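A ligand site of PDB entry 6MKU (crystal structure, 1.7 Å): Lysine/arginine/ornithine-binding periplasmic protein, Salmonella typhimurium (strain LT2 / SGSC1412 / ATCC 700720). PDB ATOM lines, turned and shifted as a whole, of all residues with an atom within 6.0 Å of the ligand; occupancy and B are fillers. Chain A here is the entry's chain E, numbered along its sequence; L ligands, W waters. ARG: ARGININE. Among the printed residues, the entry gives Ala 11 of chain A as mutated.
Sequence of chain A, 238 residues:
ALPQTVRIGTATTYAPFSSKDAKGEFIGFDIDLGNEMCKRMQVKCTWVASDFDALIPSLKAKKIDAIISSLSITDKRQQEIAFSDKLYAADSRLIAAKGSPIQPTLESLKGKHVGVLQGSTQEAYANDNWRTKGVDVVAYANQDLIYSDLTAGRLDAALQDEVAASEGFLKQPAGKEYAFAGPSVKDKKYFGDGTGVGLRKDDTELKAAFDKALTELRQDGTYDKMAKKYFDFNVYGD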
ATOM      1  N   THR A  10       9.821  -4.812 -19.122  1.00  0.00           N
ATOM      2  CA  THR A  10      10.353  -4.630 -17.790  1.00  0.00           C
ATOM      3  C   THR A  10      11.020  -3.276 -17.744  1.00  0.00           C
ATOM      4  O   THR A  10      11.403  -2.738 -18.785  1.00  0.00           O
ATOM      5  CB  THR A  10      11.325  -5.773 -17.398  1.00  0.00           C
ATOM      6  OG1 THR A  10      11.658  -5.697 -16.008  1.00  0.00           O
ATOM      7  CG2 THR A  10      12.616  -5.755 -18.252  1.00  0.00           C
ATOM      8  N   ALA A  11      11.115  -2.692 -16.557  1.00  0.00           N
ATOM      9  CA  ALA A  11      11.778  -1.399 -16.444  1.00  0.00           C
ATOM     10  C   ALA A  11      13.087  -1.616 -15.697  1.00  0.00           C
ATOM     11  O   ALA A  11      13.111  -1.875 -14.500  1.00  0.00           O
ATOM     12  CB  ALA A  11      10.892  -0.399 -15.738  1.00  0.00           C
ATOM     13  N   THR A  12      14.177  -1.509 -16.444  1.00  0.00           N
ATOM     14  CA  THR A  12      15.464  -2.072 -16.055  1.00  0.00           C
ATOM     15  C   THR A  12      16.327  -1.111 -15.246  1.00  0.00           C
ATOM     16  O   THR A  12      17.522  -0.947 -15.507  1.00  0.00           O
ATOM     17  CB  THR A  12      16.257  -2.495 -17.294  1.00  0.00           C
ATOM     18  OG1 THR A  12      16.345  -1.384 -18.198  1.00  0.00           O
ATOM     19  CG2 THR A  12      15.540  -3.632 -18.014  1.00  0.00           C
ATOM     20  N   THR A  13      15.705  -0.490 -14.247  1.00  0.00           N
ATOM     21  CA  THR A  13      16.356   0.445 -13.328  1.00  0.00           C
ATOM     22  C   THR A  13      15.810   0.187 -11.917  1.00  0.00           C
ATOM     23  O   THR A  13      15.449   1.102 -11.188  1.00  0.00           O
ATOM     24  CB  THR A  13      16.128   1.911 -13.755  1.00  0.00           C
ATOM     25  OG1 THR A  13      14.737   2.118 -14.035  1.00  0.00           O
ATOM     26  CG2 THR A  13      16.909   2.228 -15.002  1.00  0.00           C
ATOM     27  N   TYR A  14      15.766  -1.093 -11.535  1.00  0.00           N
ATOM     28  CA  TYR A  14      15.196  -1.482 -10.250  1.00  0.00           C
ATOM     29  C   TYR A  14      15.900  -2.729  -9.737  1.00  0.00           C
ATOM     30  O   TYR A  14      15.287  -3.772  -9.495  1.00  0.00           O
ATOM     31  CB  TYR A  14      13.691  -1.759 -10.397  1.00  0.00           C
ATOM     32  CG  TYR A  14      12.809  -1.204  -9.279  1.00  0.00           C
ATOM     33  CD1 TYR A  14      12.691   0.157  -9.072  1.00  0.00           C
ATOM     34  CD2 TYR A  14      12.084  -2.055  -8.466  1.00  0.00           C
ATOM     35  CE1 TYR A  14      11.856   0.674  -8.081  1.00  0.00           C
ATOM     36  CE2 TYR A  14      11.250  -1.574  -7.479  1.00  0.00           C
ATOM     37  CZ  TYR A  14      11.146  -0.205  -7.288  1.00  0.00           C
ATOM     38  OH  TYR A  14      10.313   0.262  -6.301  1.00  0.00           O
ATOM     39  N   SER A  18      15.418  -5.964 -11.615  1.00  0.00           N
ATOM     40  CA  SER A  18      15.551  -5.722 -13.049  1.00  0.00           C
ATOM     41  C   SER A  18      16.503  -4.551 -13.281  1.00  0.00           C
ATOM     42  O   SER A  18      16.218  -3.433 -12.879  1.00  0.00           O
ATOM     43  CB  SER A  18      14.193  -5.440 -13.688  1.00  0.00           C
ATOM     44  OG  SER A  18      14.287  -5.266 -15.100  1.00  0.00           O
ATOM     45  N   ASP A  30      13.774 -10.751 -11.394  1.00  0.00           N
ATOM     46  CA  ASP A  30      12.649 -10.759 -12.319  1.00  0.00           C
ATOM     47  C   ASP A  30      13.029 -11.477 -13.602  1.00  0.00           C
ATOM     48  O   ASP A  30      12.246 -12.241 -14.156  1.00  0.00           O
ATOM     49  CB  ASP A  30      12.198  -9.344 -12.682  1.00  0.00           C
ATOM     50  CG  ASP A  30      11.289  -8.712 -11.641  1.00  0.00           C
ATOM     51  OD1 ASP A  30      10.791  -9.415 -10.728  1.00  0.00           O
ATOM     52  OD2 ASP A  30      11.032  -7.495 -11.770  1.00  0.00           O
ATOM     53  N   PHE A  52       8.887   2.523 -16.491  1.00  0.00           N
ATOM     54  CA  PHE A  52       7.915   1.724 -15.743  1.00  0.00           C
ATOM     55  C   PHE A  52       6.470   2.091 -16.094  1.00  0.00           C
ATOM     56  O   PHE A  52       5.622   1.214 -16.289  1.00  0.00           O
ATOM     57  CB  PHE A  52       8.148   1.859 -14.234  1.00  0.00           C
ATOM     58  CG  PHE A  52       7.216   1.012 -13.421  1.00  0.00           C
ATOM     59  CD1 PHE A  52       7.414  -0.348 -13.298  1.00  0.00           C
ATOM     60  CD2 PHE A  52       6.119   1.582 -12.788  1.00  0.00           C
ATOM     61  CE1 PHE A  52       6.553  -1.141 -12.556  1.00  0.00           C
ATOM     62  CE2 PHE A  52       5.250   0.797 -12.018  1.00  0.00           C
ATOM     63  CZ  PHE A  52       5.478  -0.567 -11.903  1.00  0.00           C
ATOM     64  N   LEU A  55       4.583   0.453 -19.070  1.00  0.00           N
ATOM     65  CA  LEU A  55       4.387  -0.993 -19.111  1.00  0.00           C
ATOM     66  C   LEU A  55       2.907  -1.396 -19.272  1.00  0.00           C
ATOM     67  O   LEU A  55       2.545  -2.160 -20.185  1.00  0.00           O
ATOM     68  CB  LEU A  55       4.972  -1.623 -17.850  1.00  0.00           C
ATOM     69  CG  LEU A  55       6.499  -1.621 -17.810  1.00  0.00           C
ATOM     70  CD1 LEU A  55       7.011  -2.114 -16.495  1.00  0.00           C
ATOM     71  CD2 LEU A  55       7.061  -2.466 -18.950  1.00  0.00           C
ATOM     72  N   SER A  69       8.186  -6.920 -13.652  1.00  0.00           N
ATOM     73  CA  SER A  69       8.855  -5.656 -13.328  1.00  0.00           C
ATOM     74  C   SER A  69       8.496  -5.199 -11.925  1.00  0.00           C
ATOM     75  O   SER A  69       8.191  -4.024 -11.713  1.00  0.00           O
ATOM     76  CB  SER A  69       8.459  -4.575 -14.344  1.00  0.00           C
ATOM     77  OG  SER A  69       9.439  -3.562 -14.426  1.00  0.00           O
ATOM     78  N   SER A  70       8.554  -6.133 -10.977  1.00  0.00           N
ATOM     79  CA  SER A  70       8.136  -5.863  -9.607  1.00  0.00           C
ATOM     80  C   SER A  70       6.734  -5.240  -9.593  1.00  0.00           C
ATOM     81  O   SER A  70       6.453  -4.368  -8.789  1.00  0.00           O
ATOM     82  CB  SER A  70       9.144  -4.921  -8.909  1.00  0.00           C
ATOM     83  OG  SER A  70      10.372  -5.555  -8.639  1.00  0.00           O
ATOM     84  N   LEU A  71       5.885  -5.691 -10.506  1.00  0.00           N
ATOM     85  CA  LEU A  71       4.555  -5.097 -10.658  1.00  0.00           C
ATOM     86  C   LEU A  71       3.584  -5.583  -9.570  1.00  0.00           C
ATOM     87  O   LEU A  71       3.104  -6.727  -9.599  1.00  0.00           O
ATOM     88  CB  LEU A  71       3.982  -5.409 -12.040  1.00  0.00           C
ATOM     89  CG  LEU A  71       2.720  -4.653 -12.477  1.00  0.00           C
ATOM     90  CD1 LEU A  71       3.028  -3.183 -12.727  1.00  0.00           C
ATOM     91  CD2 LEU A  71       2.067  -5.307 -13.707  1.00  0.00           C
ATOM     92  N   SER A  72       3.323  -4.706  -8.606  1.00  0.00           N
ATOM     93  CA  SER A  72       2.446  -5.027  -7.469  1.00  0.00           C
ATOM     94  C   SER A  72       1.013  -5.360  -7.867  1.00  0.00           C
ATOM     95  O   SER A  72       0.409  -4.693  -8.701  1.00  0.00           O
ATOM     96  CB  SER A  72       2.440  -3.846  -6.474  1.00  0.00           C
ATOM     97  OG  SER A  72       3.668  -3.798  -5.789  1.00  0.00           O
ATOM     98  N   ARG A  77      -5.257  -2.074 -10.218  1.00  0.00           N
ATOM     99  CA  ARG A  77      -4.703  -2.605 -11.467  1.00  0.00           C
ATOM    100  C   ARG A  77      -5.502  -3.782 -11.991  1.00  0.00           C
ATOM    101  O   ARG A  77      -5.559  -4.028 -13.202  1.00  0.00           O
ATOM    102  CB  ARG A  77      -3.246  -3.004 -11.305  1.00  0.00           C
ATOM    103  CG  ARG A  77      -2.340  -1.813 -11.247  1.00  0.00           C
ATOM    104  CD  ARG A  77      -0.931  -2.228 -10.886  1.00  0.00           C
ATOM    105  NE  ARG A  77      -0.037  -1.086 -10.897  1.00  0.00           N
ATOM    106  CZ  ARG A  77       1.146  -1.050 -10.316  1.00  0.00           C
ATOM    107  NH1 ARG A  77       1.589  -2.111  -9.644  1.00  0.00           N
ATOM    108  NH2 ARG A  77       1.885   0.047 -10.406  1.00  0.00           N
ATOM    109  N   ALA A  90       6.325  -7.446  -1.634  1.00  0.00           N
ATOM    110  CA  ALA A  90       6.935  -6.135  -1.819  1.00  0.00           C
ATOM    111  C   ALA A  90       6.315  -5.057  -0.953  1.00  0.00           C
ATOM    112  O   ALA A  90       5.236  -4.556  -1.245  1.00  0.00           O
ATOM    113  CB  ALA A  90       6.871  -5.712  -3.290  1.00  0.00           C
ATOM    114  N   LEU A 117       8.589   6.989  -8.163  1.00  0.00           N
ATOM    115  CA  LEU A 117       8.608   6.556  -9.554  1.00  0.00           C
ATOM    116  C   LEU A 117       7.266   6.801 -10.254  1.00  0.00           C
ATOM    117  O   LEU A 117       6.214   6.412  -9.751  1.00  0.00           O
ATOM    118  CB  LEU A 117       8.992   5.087  -9.609  1.00  0.00           C
ATOM    119  CG  LEU A 117       8.930   4.369 -10.943  1.00  0.00           C
ATOM    120  CD1 LEU A 117      10.031   4.865 -11.876  1.00  0.00           C
ATOM    121  CD2 LEU A 117       9.019   2.868 -10.686  1.00  0.00           C
ATOM    122  N   GLY A 119       4.111   6.323 -12.279  1.00  0.00           N
ATOM    123  CA  GLY A 119       3.348   5.134 -12.594  1.00  0.00           C
ATOM    124  C   GLY A 119       3.302   4.098 -11.479  1.00  0.00           C
ATOM    125  O   GLY A 119       2.646   3.069 -11.621  1.00  0.00           O
ATOM    126  N   SER A 120       4.001   4.365 -10.371  1.00  0.00           N
ATOM    127  CA  SER A 120       4.116   3.390  -9.287  1.00  0.00           C
ATOM    128  C   SER A 120       3.011   3.506  -8.244  1.00  0.00           C
ATOM    129  O   SER A 120       2.346   4.532  -8.124  1.00  0.00           O
ATOM    130  CB  SER A 120       5.469   3.518  -8.592  1.00  0.00           C
ATOM    131  OG  SER A 120       5.519   4.693  -7.805  1.00  0.00           O
ATOM    132  N   THR A 121       2.843   2.420  -7.478  1.00  0.00           N
ATOM    133  CA  THR A 121       1.991   2.448  -6.285  1.00  0.00           C
ATOM    134  C   THR A 121       2.489   3.496  -5.313  1.00  0.00           C
ATOM    135  O   THR A 121       1.700   4.108  -4.594  1.00  0.00           O
ATOM    136  CB  THR A 121       1.981   1.100  -5.564  1.00  0.00           C
ATOM    137  OG1 THR A 121       3.335   0.677  -5.343  1.00  0.00           O
ATOM    138  CG2 THR A 121       1.262   0.056  -6.376  1.00  0.00           C
ATOM    139  N   GLN A 122       3.797   3.727  -5.279  1.00  0.00           N
ATOM    140  CA  GLN A 122       4.345   4.727  -4.368  1.00  0.00           C
ATOM    141  C   GLN A 122       3.951   6.130  -4.795  1.00  0.00           C
ATOM    142  O   GLN A 122       3.736   7.005  -3.953  1.00  0.00           O
ATOM    143  CB  GLN A 122       5.861   4.595  -4.265  1.00  0.00           C
ATOM    144  CG  GLN A 122       6.324   3.340  -3.547  1.00  0.00           C
ATOM    145  CD  GLN A 122       6.497   2.155  -4.471  1.00  0.00           C
ATOM    146  OE1 GLN A 122       6.453   2.302  -5.699  1.00  0.00           O
ATOM    147  NE2 GLN A 122       6.721   0.983  -3.900  1.00  0.00           N
ATOM    148  N   GLN A 143      13.835   4.910 -11.432  1.00  0.00           N
ATOM    149  CA  GLN A 143      14.307   4.909 -10.052  1.00  0.00           C
ATOM    150  C   GLN A 143      15.784   5.330  -9.932  1.00  0.00           C
ATOM    151  O   GLN A 143      16.185   5.843  -8.887  1.00  0.00           O
ATOM    152  CB  GLN A 143      14.113   3.519  -9.420  1.00  0.00           C
ATOM    153  CG  GLN A 143      14.443   3.423  -7.917  1.00  0.00           C
ATOM    154  CD  GLN A 143      13.476   4.182  -7.023  1.00  0.00           C
ATOM    155  OE1 GLN A 143      12.264   4.185  -7.260  1.00  0.00           O
ATOM    156  NE2 GLN A 143      14.009   4.838  -5.987  1.00  0.00           N
ATOM    157  N   ASP A 161      10.009   0.323  -3.441  1.00  0.00           N
ATOM    158  CA  ASP A 161       9.953  -0.992  -2.797  1.00  0.00           C
ATOM    159  C   ASP A 161      11.159  -1.161  -1.877  1.00  0.00           C
ATOM    160  O   ASP A 161      12.284  -0.803  -2.214  1.00  0.00           O
ATOM    161  CB  ASP A 161       9.912  -2.131  -3.829  1.00  0.00           C
ATOM    162  CG  ASP A 161       8.601  -2.224  -4.609  1.00  0.00           C
ATOM    163  OD1 ASP A 161       7.593  -1.593  -4.219  1.00  0.00           O
ATOM    164  OD2 ASP A 161       8.564  -2.948  -5.631  1.00  0.00           O
ATOM    165  N   THR A 195       4.082  -8.947  -5.844  1.00  0.00           N
ATOM    166  CA  THR A 195       4.146  -8.663  -7.270  1.00  0.00           C
ATOM    167  C   THR A 195       3.779  -9.886  -8.097  1.00  0.00           C
ATOM    168  O   THR A 195       3.818 -11.006  -7.602  1.00  0.00           O
ATOM    169  CB  THR A 195       5.565  -8.190  -7.701  1.00  0.00           C
ATOM    170  OG1 THR A 195       6.479  -9.299  -7.694  1.00  0.00           O
ATOM    171  CG2 THR A 195       6.089  -7.140  -6.743  1.00  0.00           C
HETATM  172  N   ARG L   1       6.006  -2.313  -6.884  1.00  0.00           N
HETATM  173  CA  ARG L   1       5.842  -0.918  -7.313  1.00  0.00           C
HETATM  174  C   ARG L   1       4.687  -0.833  -8.298  1.00  0.00           C
HETATM  175  O   ARG L   1       4.193  -1.869  -8.747  1.00  0.00           O
HETATM  176  CB  ARG L   1       7.125  -0.375  -7.955  1.00  0.00           C
HETATM  177  CG  ARG L   1       7.685  -1.294  -9.028  1.00  0.00           C
HETATM  178  CD  ARG L   1       8.696  -0.599  -9.929  1.00  0.00           C
HETATM  179  NE  ARG L   1       9.417  -1.555 -10.761  1.00  0.00           N
HETATM  180  CZ  ARG L   1      10.353  -1.233 -11.646  1.00  0.00           C
HETATM  181  NH1 ARG L   1      10.682   0.038 -11.827  1.00  0.00           N
HETATM  182  NH2 ARG L   1      10.977  -2.179 -12.362  1.00  0.00           N
HETATM  183  OXT ARG L   1       4.248   0.253  -8.691  1.00  0.00           O
HETATM  184  O   HOH W   1      12.407   2.353 -12.596  1.00  0.00           O
HETATM  185  O   HOH W   2      11.683  -4.783 -11.191  1.00  0.00           O
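Water W2 lies within hydrogen-bond range of OD2 of Asp 30, NH2 of the ligand and OG of Ser 70.
Water W1 lies within hydrogen-bond range of the side-chain hydroxyl (OG1) of Thr 13, a nitrogen (NH1) of the ligand and the backbone NH (N) of Gln 143.
The backbone carbonyl oxygen of Ser 72 lies within hydrogen-bond range of the guanidinium group of Arg 77 (3.0 Å).
The guanidinium group of Arg 77 is in hydrogen-bond range of the backbone carbonyl oxygen of Gly 119.
The side-chain hydroxyl of Ser 69 sits at hydrogen-bond distance from the backbone NH of Ala 11.
The backbone NH (N) of Asp 161 is in hydrogen-bond range of the side-chain hydroxyl (OH) of Tyr 14, 2.9 Å away.
The backbone carbonyl oxygen (O) of Leu 117 sits at hydrogen-bond distance from the side-chain hydroxyl (OG) of Ser 120 (2.7 Å).
N of Ser 70 is in hydrogen-bond range of OD2 of Asp 30 (2.9 Å).
The side-chain hydroxyl of Ser 69 sits at hydrogen-bond distance from the side-chain hydroxyl of Thr 10, 3.5 Å away.
OD1 of Asp 161 is in hydrogen-bond range of NE2 of Gln 122 (2.7 Å).
Residues that only touch the ligand: Ser 120, Tyr 14, Phe 52, Leu 117, Gln 122 and Leu 71.
Hydrophobic or aromatic side chains within 4 Å of the ligand: Ala 11, Tyr 14, Phe 52 and Leu 117.
Within 4 Å of the ligand: Ala 11, Tyr 14, Phe 52, Ser 69, Ser 70, Leu 71, Ser 72, Arg 77, Leu 117, Ser 120, Thr 121, Gln 122 and Asp 161.
The nearest printed residue that does not touch the ligand is Gly 119 (4.4 Å).
A nitrogen (N) of the ligand is in salt-bridge range of the side-chain carboxylate of Asp 161 (2.9 Å).
The backbone carbonyl oxygen (O) of Ala 11 lies within hydrogen-bond range of a nitrogen (NH2) of the ligand (3.0 Å).
NH2 of the ligand sits at hydrogen-bond distance from OG of Ser 69 (2.9 Å).
The backbone NH (N) of Thr 121 is in hydrogen-bond range of an oxygen (OXT) of the ligand (2.9 Å).
N of Ser 72 lies within hydrogen-bond range of O of the ligand, at 3.0 Å.
N of the ligand sits at hydrogen-bond distance from OG of Ser 72, at 3.0 Å.
An oxygen (O) of the ligand lies within salt-bridge range of the guanidinium group of Arg 77 (2.8 Å).
The backbone carbonyl oxygen (O) of Ser 69 is in hydrogen-bond range of a nitrogen (NE) of the ligand (2.9 Å).
OXT of the ligand lies within hydrogen-bond range of OG1 of Thr 121.
A nitrogen (N) of the ligand lies within hydrogen-bond range of the backbone carbonyl oxygen (O) of Ser 70 (2.8 Å).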
